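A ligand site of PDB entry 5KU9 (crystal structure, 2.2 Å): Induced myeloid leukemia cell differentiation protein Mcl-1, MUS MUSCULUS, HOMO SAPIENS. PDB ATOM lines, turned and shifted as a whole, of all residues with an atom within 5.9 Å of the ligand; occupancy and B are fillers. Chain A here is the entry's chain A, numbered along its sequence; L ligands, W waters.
OG of Ser 90 is in hydrogen-bond range of ND1 of His 87 (2.8 Å).
The side-chain carboxylate (OD2) of Asp 91 lies within salt-bridge range of the guanidinium group (NH1) of Arg 98 (2.7 Å).
The backbone carbonyl oxygen (O) of Val 88 lies within hydrogen-bond range of the guanidinium group (NH2) of Arg 98 (2.7 Å).
Merely in contact with the ligand: His 59, Ala 62, Phe 63, Met 66, Val 84, Met 85, Val 88, Asp 91, Arg 98, Thr 101, Leu 102 and Phe 105.
Hydrophobic or aromatic side chains that line the ligand: His 59, Ala 62, Phe 63, Met 66, Val 84, His 87 and Phe 105.
Within 4 Å of the ligand: His 59, Ala 62, Phe 63, Met 66, Val 84, Met 85, His 87, Val 88, Ser 90, Asp 91, Arg 98, Thr 101, Leu 102 and Phe 105.
The nearest printed residue that does not touch the ligand is Lys 69 (4.8 Å).
The side-chain hydroxyl of Ser 90 lies within hydrogen-bond range of a nitrogen (N1) of the ligand, at 3.1 Å.
O of His 87 sits close to N1 of the ligand, at 3.2 Å.
Water W5 bridges an oxygen (O3) of the ligand (2.9 Å) and the side-chain amino group (NZ) of Lys 69 (3.2 Å).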
ATOM      1  N   HIS A  59     -14.521   7.112  36.745  1.00  0.00           N
ATOM      2  CA  HIS A  59     -15.410   5.987  36.413  1.00  0.00           C
ATOM      3  C   HIS A  59     -15.834   5.147  37.632  1.00  0.00           C
ATOM      4  O   HIS A  59     -16.331   4.042  37.446  1.00  0.00           O
ATOM      5  CB  HIS A  59     -14.711   5.062  35.390  1.00  0.00           C
ATOM      6  CG  HIS A  59     -14.436   5.682  34.060  1.00  0.00           C
ATOM      7  ND1 HIS A  59     -15.391   6.420  33.394  1.00  0.00           N
ATOM      8  CD2 HIS A  59     -13.342   5.571  33.269  1.00  0.00           C
ATOM      9  CE1 HIS A  59     -14.839   6.775  32.247  1.00  0.00           C
ATOM     10  NE2 HIS A  59     -13.607   6.262  32.132  1.00  0.00           N
ATOM     11  N   ALA A  62     -19.373   3.706  37.522  1.00  0.00           N
ATOM     12  CA  ALA A  62     -19.386   2.684  36.457  1.00  0.00           C
ATOM     13  C   ALA A  62     -18.646   1.400  36.891  1.00  0.00           C
ATOM     14  O   ALA A  62     -19.203   0.320  36.753  1.00  0.00           O
ATOM     15  CB  ALA A  62     -18.788   3.256  35.176  1.00  0.00           C
ATOM     16  N   PHE A  63     -17.432   1.519  37.497  1.00  0.00           N
ATOM     17  CA  PHE A  63     -16.647   0.394  38.030  1.00  0.00           C
ATOM     18  C   PHE A  63     -17.387  -0.354  39.106  1.00  0.00           C
ATOM     19  O   PHE A  63     -17.468  -1.576  39.032  1.00  0.00           O
ATOM     20  CB  PHE A  63     -15.245   0.829  38.530  1.00  0.00           C
ATOM     21  CG  PHE A  63     -14.225   1.165  37.472  1.00  0.00           C
ATOM     22  CD1 PHE A  63     -14.486   0.921  36.118  1.00  0.00           C
ATOM     23  CD2 PHE A  63     -13.029   1.783  37.809  1.00  0.00           C
ATOM     24  CE1 PHE A  63     -13.566   1.292  35.136  1.00  0.00           C
ATOM     25  CE2 PHE A  63     -12.104   2.142  36.825  1.00  0.00           C
ATOM     26  CZ  PHE A  63     -12.379   1.897  35.492  1.00  0.00           C
ATOM     27  N   MET A  66     -20.182  -2.307  37.495  1.00  0.00           N
ATOM     28  CA  MET A  66     -19.633  -3.530  36.865  1.00  0.00           C
ATOM     29  C   MET A  66     -19.333  -4.622  37.900  1.00  0.00           C
ATOM     30  O   MET A  66     -19.802  -5.746  37.714  1.00  0.00           O
ATOM     31  CB  MET A  66     -18.362  -3.229  36.090  1.00  0.00           C
ATOM     32  CG  MET A  66     -18.575  -2.407  34.855  1.00  0.00           C
ATOM     33  SD  MET A  66     -17.024  -2.288  33.961  1.00  0.00           S
ATOM     34  CE  MET A  66     -16.917  -3.868  33.287  1.00  0.00           C
ATOM     35  N   LYS A  69     -22.449  -6.503  39.267  1.00  0.00           N
ATOM     36  CA  LYS A  69     -23.027  -7.471  38.320  1.00  0.00           C
ATOM     37  C   LYS A  69     -22.152  -8.704  38.140  1.00  0.00           C
ATOM     38  O   LYS A  69     -22.672  -9.776  37.806  1.00  0.00           O
ATOM     39  CB  LYS A  69     -23.261  -6.801  36.952  1.00  0.00           C
ATOM     40  CG  LYS A  69     -24.547  -5.980  36.866  1.00  0.00           C
ATOM     41  CD  LYS A  69     -24.450  -4.854  35.828  1.00  0.00           C
ATOM     42  CE  LYS A  69     -24.890  -5.272  34.446  1.00  0.00           C
ATOM     43  NZ  LYS A  69     -24.519  -4.255  33.430  1.00  0.00           N
ATOM     44  N   LEU A  81     -13.209 -12.878  33.609  1.00  0.00           N
ATOM     45  CA  LEU A  81     -13.261 -11.433  33.369  1.00  0.00           C
ATOM     46  C   LEU A  81     -12.797 -11.089  31.962  1.00  0.00           C
ATOM     47  O   LEU A  81     -13.084  -9.990  31.482  1.00  0.00           O
ATOM     48  CB  LEU A  81     -12.445 -10.620  34.407  1.00  0.00           C
ATOM     49  CG  LEU A  81     -12.989 -10.522  35.818  1.00  0.00           C
ATOM     50  CD1 LEU A  81     -12.014  -9.791  36.720  1.00  0.00           C
ATOM     51  CD2 LEU A  81     -14.299  -9.804  35.872  1.00  0.00           C
ATOM     52  N   ARG A  83     -13.895 -12.125  29.069  1.00  0.00           N
ATOM     53  CA  ARG A  83     -15.069 -11.958  28.187  1.00  0.00           C
ATOM     54  C   ARG A  83     -15.613 -10.530  28.260  1.00  0.00           C
ATOM     55  O   ARG A  83     -16.111  -9.993  27.266  1.00  0.00           O
ATOM     56  CB  ARG A  83     -16.184 -12.982  28.556  1.00  0.00           C
ATOM     57  CG  ARG A  83     -15.711 -14.447  28.556  1.00  0.00           C
ATOM     58  CD  ARG A  83     -16.823 -15.472  28.760  1.00  0.00           C
ATOM     59  NE  ARG A  83     -17.194 -16.123  27.506  1.00  0.00           N
ATOM     60  CZ  ARG A  83     -18.016 -17.174  27.407  1.00  0.00           C
ATOM     61  NH1 ARG A  83     -18.568 -17.705  28.497  1.00  0.00           N
ATOM     62  NH2 ARG A  83     -18.292 -17.704  26.223  1.00  0.00           N
ATOM     63  N   VAL A  84     -15.507  -9.921  29.449  1.00  0.00           N
ATOM     64  CA  VAL A  84     -15.931  -8.556  29.745  1.00  0.00           C
ATOM     65  C   VAL A  84     -14.899  -7.529  29.198  1.00  0.00           C
ATOM     66  O   VAL A  84     -15.273  -6.614  28.452  1.00  0.00           O
ATOM     67  CB  VAL A  84     -16.184  -8.451  31.284  1.00  0.00           C
ATOM     68  CG1 VAL A  84     -16.145  -7.022  31.789  1.00  0.00           C
ATOM     69  CG2 VAL A  84     -17.511  -9.117  31.674  1.00  0.00           C
ATOM     70  N   MET A  85     -13.624  -7.706  29.548  1.00  0.00           N
ATOM     71  CA  MET A  85     -12.487  -6.858  29.183  1.00  0.00           C
ATOM     72  C   MET A  85     -12.360  -6.560  27.696  1.00  0.00           C
ATOM     73  O   MET A  85     -11.995  -5.444  27.355  1.00  0.00           O
ATOM     74  CB  MET A  85     -11.169  -7.465  29.686  1.00  0.00           C
ATOM     75  CG  MET A  85     -10.976  -7.440  31.179  1.00  0.00           C
ATOM     76  SD  MET A  85      -9.390  -8.297  31.515  1.00  0.00           S
ATOM     77  CE  MET A  85      -9.572  -8.557  33.212  1.00  0.00           C
ATOM     78  N   ILE A  86     -12.617  -7.548  26.817  1.00  0.00           N
ATOM     79  CA  ILE A  86     -12.494  -7.308  25.356  1.00  0.00           C
ATOM     80  C   ILE A  86     -13.451  -6.224  24.859  1.00  0.00           C
ATOM     81  O   ILE A  86     -13.185  -5.613  23.827  1.00  0.00           O
ATOM     82  CB  ILE A  86     -12.592  -8.578  24.483  1.00  0.00           C
ATOM     83  CG1 ILE A  86     -13.861  -9.394  24.784  1.00  0.00           C
ATOM     84  CG2 ILE A  86     -11.319  -9.429  24.584  1.00  0.00           C
ATOM     85  CD1 ILE A  86     -14.586  -9.773  23.555  1.00  0.00           C
ATOM     86  N   HIS A  87     -14.550  -5.995  25.602  1.00  0.00           N
ATOM     87  CA  HIS A  87     -15.541  -4.996  25.254  1.00  0.00           C
ATOM     88  C   HIS A  87     -15.060  -3.564  25.525  1.00  0.00           C
ATOM     89  O   HIS A  87     -15.708  -2.652  25.042  1.00  0.00           O
ATOM     90  CB  HIS A  87     -16.884  -5.306  25.878  1.00  0.00           C
ATOM     91  CG  HIS A  87     -17.540  -6.449  25.176  1.00  0.00           C
ATOM     92  ND1 HIS A  87     -17.892  -6.372  23.843  1.00  0.00           N
ATOM     93  CD2 HIS A  87     -17.748  -7.707  25.616  1.00  0.00           C
ATOM     94  CE1 HIS A  87     -18.362  -7.558  23.532  1.00  0.00           C
ATOM     95  NE2 HIS A  87     -18.332  -8.389  24.569  1.00  0.00           N
ATOM     96  N   VAL A  88     -13.869  -3.355  26.136  1.00  0.00           N
ATOM     97  CA  VAL A  88     -13.329  -1.988  26.244  1.00  0.00           C
ATOM     98  C   VAL A  88     -12.927  -1.529  24.821  1.00  0.00           C
ATOM     99  O   VAL A  88     -12.808  -0.337  24.571  1.00  0.00           O
ATOM    100  CB  VAL A  88     -12.151  -1.828  27.285  1.00  0.00           C
ATOM    101  CG1 VAL A  88     -10.876  -2.476  26.779  1.00  0.00           C
ATOM    102  CG2 VAL A  88     -11.887  -0.360  27.622  1.00  0.00           C
ATOM    103  N   PHE A  89     -12.746  -2.483  23.877  1.00  0.00           N
ATOM    104  CA  PHE A  89     -12.348  -2.177  22.509  1.00  0.00           C
ATOM    105  C   PHE A  89     -13.369  -2.578  21.445  1.00  0.00           C
ATOM    106  O   PHE A  89     -13.081  -2.421  20.252  1.00  0.00           O
ATOM    107  CB  PHE A  89     -11.011  -2.902  22.212  1.00  0.00           C
ATOM    108  CG  PHE A  89      -9.838  -2.560  23.122  1.00  0.00           C
ATOM    109  CD1 PHE A  89      -9.385  -1.250  23.236  1.00  0.00           C
ATOM    110  CD2 PHE A  89      -9.168  -3.560  23.830  1.00  0.00           C
ATOM    111  CE1 PHE A  89      -8.294  -0.946  24.061  1.00  0.00           C
ATOM    112  CE2 PHE A  89      -8.073  -3.259  24.634  1.00  0.00           C
ATOM    113  CZ  PHE A  89      -7.642  -1.951  24.752  1.00  0.00           C
ATOM    114  N   SER A  90     -14.533  -3.134  21.838  1.00  0.00           N
ATOM    115  CA  SER A  90     -15.481  -3.678  20.866  1.00  0.00           C
ATOM    116  C   SER A  90     -16.236  -2.626  20.023  1.00  0.00           C
ATOM    117  O   SER A  90     -16.864  -3.014  19.045  1.00  0.00           O
ATOM    118  CB  SER A  90     -16.446  -4.662  21.513  1.00  0.00           C
ATOM    119  OG  SER A  90     -17.276  -3.992  22.456  1.00  0.00           O
ATOM    120  N   ASP A  91     -16.103  -1.312  20.324  1.00  0.00           N
ATOM    121  CA  ASP A  91     -16.740  -0.291  19.486  1.00  0.00           C
ATOM    122  C   ASP A  91     -15.805   0.159  18.352  1.00  0.00           C
ATOM    123  O   ASP A  91     -16.104   1.121  17.642  1.00  0.00           O
ATOM    124  CB  ASP A  91     -17.259   0.899  20.293  1.00  0.00           C
ATOM    125  CG  ASP A  91     -16.204   1.680  21.038  1.00  0.00           C
ATOM    126  OD1 ASP A  91     -15.038   1.232  21.056  1.00  0.00           O
ATOM    127  OD2 ASP A  91     -16.530   2.739  21.590  1.00  0.00           O
ATOM    128  N   ARG A  98      -8.660   4.488  26.466  1.00  0.00           N
ATOM    129  CA  ARG A  98      -9.293   3.152  26.620  1.00  0.00           C
ATOM    130  C   ARG A  98      -8.419   2.177  27.342  1.00  0.00           C
ATOM    131  O   ARG A  98      -8.895   1.403  28.158  1.00  0.00           O
ATOM    132  CB  ARG A  98      -9.588   2.545  25.250  1.00  0.00           C
ATOM    133  CG  ARG A  98     -10.800   3.108  24.577  1.00  0.00           C
ATOM    134  CD  ARG A  98     -12.090   2.955  25.396  1.00  0.00           C
ATOM    135  NE  ARG A  98     -13.107   3.705  24.683  1.00  0.00           N
ATOM    136  CZ  ARG A  98     -13.834   3.212  23.688  1.00  0.00           C
ATOM    137  NH1 ARG A  98     -14.667   3.998  23.026  1.00  0.00           N
ATOM    138  NH2 ARG A  98     -13.737   1.930  23.354  1.00  0.00           N
ATOM    139  N   THR A 101      -8.326   3.012  30.920  1.00  0.00           N
ATOM    140  CA  THR A 101      -9.609   2.635  31.525  1.00  0.00           C
ATOM    141  C   THR A 101      -9.597   1.128  31.831  1.00  0.00           C
ATOM    142  O   THR A 101      -9.986   0.738  32.915  1.00  0.00           O
ATOM    143  CB  THR A 101     -10.760   3.024  30.587  1.00  0.00           C
ATOM    144  OG1 THR A 101     -10.706   4.428  30.457  1.00  0.00           O
ATOM    145  CG2 THR A 101     -12.115   2.624  31.153  1.00  0.00           C
ATOM    146  N   LEU A 102      -9.104   0.288  30.897  1.00  0.00           N
ATOM    147  CA  LEU A 102      -8.976  -1.159  31.143  1.00  0.00           C
ATOM    148  C   LEU A 102      -8.055  -1.451  32.371  1.00  0.00           C
ATOM    149  O   LEU A 102      -8.413  -2.248  33.250  1.00  0.00           O
ATOM    150  CB  LEU A 102      -8.412  -1.865  29.898  1.00  0.00           C
ATOM    151  CG  LEU A 102      -8.029  -3.365  30.080  1.00  0.00           C
ATOM    152  CD1 LEU A 102      -9.283  -4.230  30.331  1.00  0.00           C
ATOM    153  CD2 LEU A 102      -7.258  -3.877  28.911  1.00  0.00           C
ATOM    154  N   PHE A 105      -9.655  -0.369  35.623  1.00  0.00           N
ATOM    155  CA  PHE A 105     -10.667  -1.344  36.051  1.00  0.00           C
ATOM    156  C   PHE A 105      -9.945  -2.524  36.714  1.00  0.00           C
ATOM    157  O   PHE A 105     -10.425  -3.048  37.726  1.00  0.00           O
ATOM    158  CB  PHE A 105     -11.544  -1.839  34.907  1.00  0.00           C
ATOM    159  CG  PHE A 105     -12.594  -2.820  35.388  1.00  0.00           C
ATOM    160  CD1 PHE A 105     -13.554  -2.430  36.319  1.00  0.00           C
ATOM    161  CD2 PHE A 105     -12.590  -4.135  34.962  1.00  0.00           C
ATOM    162  CE1 PHE A 105     -14.508  -3.350  36.797  1.00  0.00           C
ATOM    163  CE2 PHE A 105     -13.554  -5.048  35.418  1.00  0.00           C
ATOM    164  CZ  PHE A 105     -14.508  -4.637  36.324  1.00  0.00           C
HETATM  165  C1  LIG L   1     -20.001  -5.250  29.233  1.00  0.00           C
HETATM  166  C2  LIG L   1     -20.158  -3.748  29.194  1.00  0.00           C
HETATM  167  C3  LIG L   1     -18.969  -3.033  29.847  1.00  0.00           C
HETATM  168  C4  LIG L   1     -15.030  -0.740  30.203  1.00  0.00           C
HETATM  169  C5  LIG L   1     -14.158  -1.653  30.777  1.00  0.00           C
HETATM  170  C6  LIG L   1     -14.428  -3.001  30.688  1.00  0.00           C
HETATM  171  C7  LIG L   1     -15.561  -3.455  30.016  1.00  0.00           C
HETATM  172  C8  LIG L   1     -20.025  -1.364  31.335  1.00  0.00           C
HETATM  173  C9  LIG L   1     -20.300   0.099  31.609  1.00  0.00           C
HETATM  174  C10 LIG L   1     -18.451   1.758  31.454  1.00  0.00           C
HETATM  175  C11 LIG L   1     -17.500   0.994  32.137  1.00  0.00           C
HETATM  176  C12 LIG L   1     -16.367   1.596  32.653  1.00  0.00           C
HETATM  177  C13 LIG L   1     -16.173   2.952  32.500  1.00  0.00           C
HETATM  178  C14 LIG L   1     -19.203   4.044  30.529  1.00  0.00           C
HETATM  179  C15 LIG L   1     -19.248   3.743  29.020  1.00  0.00           C
HETATM  180  C16 LIG L   1     -19.045   2.255  28.707  1.00  0.00           C
HETATM  181  C17 LIG L   1     -20.017   1.403  29.581  1.00  0.00           C
HETATM  182  C18 LIG L   1     -19.194   0.395  25.403  1.00  0.00           C
HETATM  183  C19 LIG L   1     -16.373   1.419  25.306  1.00  0.00           C
HETATM  184  C20 LIG L   1     -15.581   3.161  27.305  1.00  0.00           C
HETATM  185  C21 LIG L   1     -16.294   3.648  26.219  1.00  0.00           C
HETATM  186  C22 LIG L   1     -16.694   2.770  25.229  1.00  0.00           C
HETATM  187 BR1  LIG L   1     -15.108   4.345  28.715  1.00  0.00          BR
HETATM  188  C23 LIG L   1     -15.250   1.834  27.408  1.00  0.00           C
HETATM  189  C24 LIG L   1     -15.642   0.969  26.400  1.00  0.00           C
HETATM  190  C25 LIG L   1     -16.904   0.441  24.282  1.00  0.00           C
HETATM  191  C26 LIG L   1     -18.025  -0.440  24.845  1.00  0.00           C
HETATM  192  N1  LIG L   1     -18.465  -1.451  23.881  1.00  0.00           N
HETATM  193  C27 LIG L   1     -19.020   0.652  26.880  1.00  0.00           C
HETATM  194  O1  LIG L   1     -18.695  -0.252  27.637  1.00  0.00           O
HETATM  195  N2  LIG L   1     -19.197   1.915  27.298  1.00  0.00           N
HETATM  196  C28 LIG L   1     -18.267   3.140  31.304  1.00  0.00           C
HETATM  197  C29 LIG L   1     -17.107   3.721  31.833  1.00  0.00           C
HETATM  198  O2  LIG L   1     -21.103   1.034  29.177  1.00  0.00           O
HETATM  199  N3  LIG L   1     -19.575   1.110  30.846  1.00  0.00           N
HETATM  200  O3  LIG L   1     -20.414  -2.216  32.124  1.00  0.00           O
HETATM  201  N4  LIG L   1     -19.376  -1.676  30.194  1.00  0.00           N
HETATM  202  O4  LIG L   1     -19.709  -5.836  30.281  1.00  0.00           O
HETATM  203  N5  LIG L   1     -20.235  -5.885  28.101  1.00  0.00           N
HETATM  204  C30 LIG L   1     -20.249  -7.339  28.011  1.00  0.00           C
HETATM  205  C31 LIG L   1     -17.757  -3.046  28.881  1.00  0.00           C
HETATM  206  C32 LIG L   1     -16.466  -2.551  29.473  1.00  0.00           C
HETATM  207 CL1  LIG L   1     -13.415  -4.154  31.503  1.00  0.00          CL
HETATM  208 CL2  LIG L   1     -12.779  -1.106  31.666  1.00  0.00          CL
HETATM  209  C33 LIG L   1     -16.178  -1.196  29.565  1.00  0.00           C
HETATM  210  O   HOH W   1     -12.298   5.695  28.668  1.00  0.00           O
HETATM  211  O   HOH W   2     -20.045  -0.516  21.969  1.00  0.00           O
HETATM  212  O   HOH W   3     -21.485   3.054  32.977  1.00  0.00           O
HETATM  213  O   HOH W   4     -20.286  -5.370  32.903  1.00  0.00           O
HETATM  214  O   HOH W   5     -22.368  -2.062  34.196  1.00  0.00           O
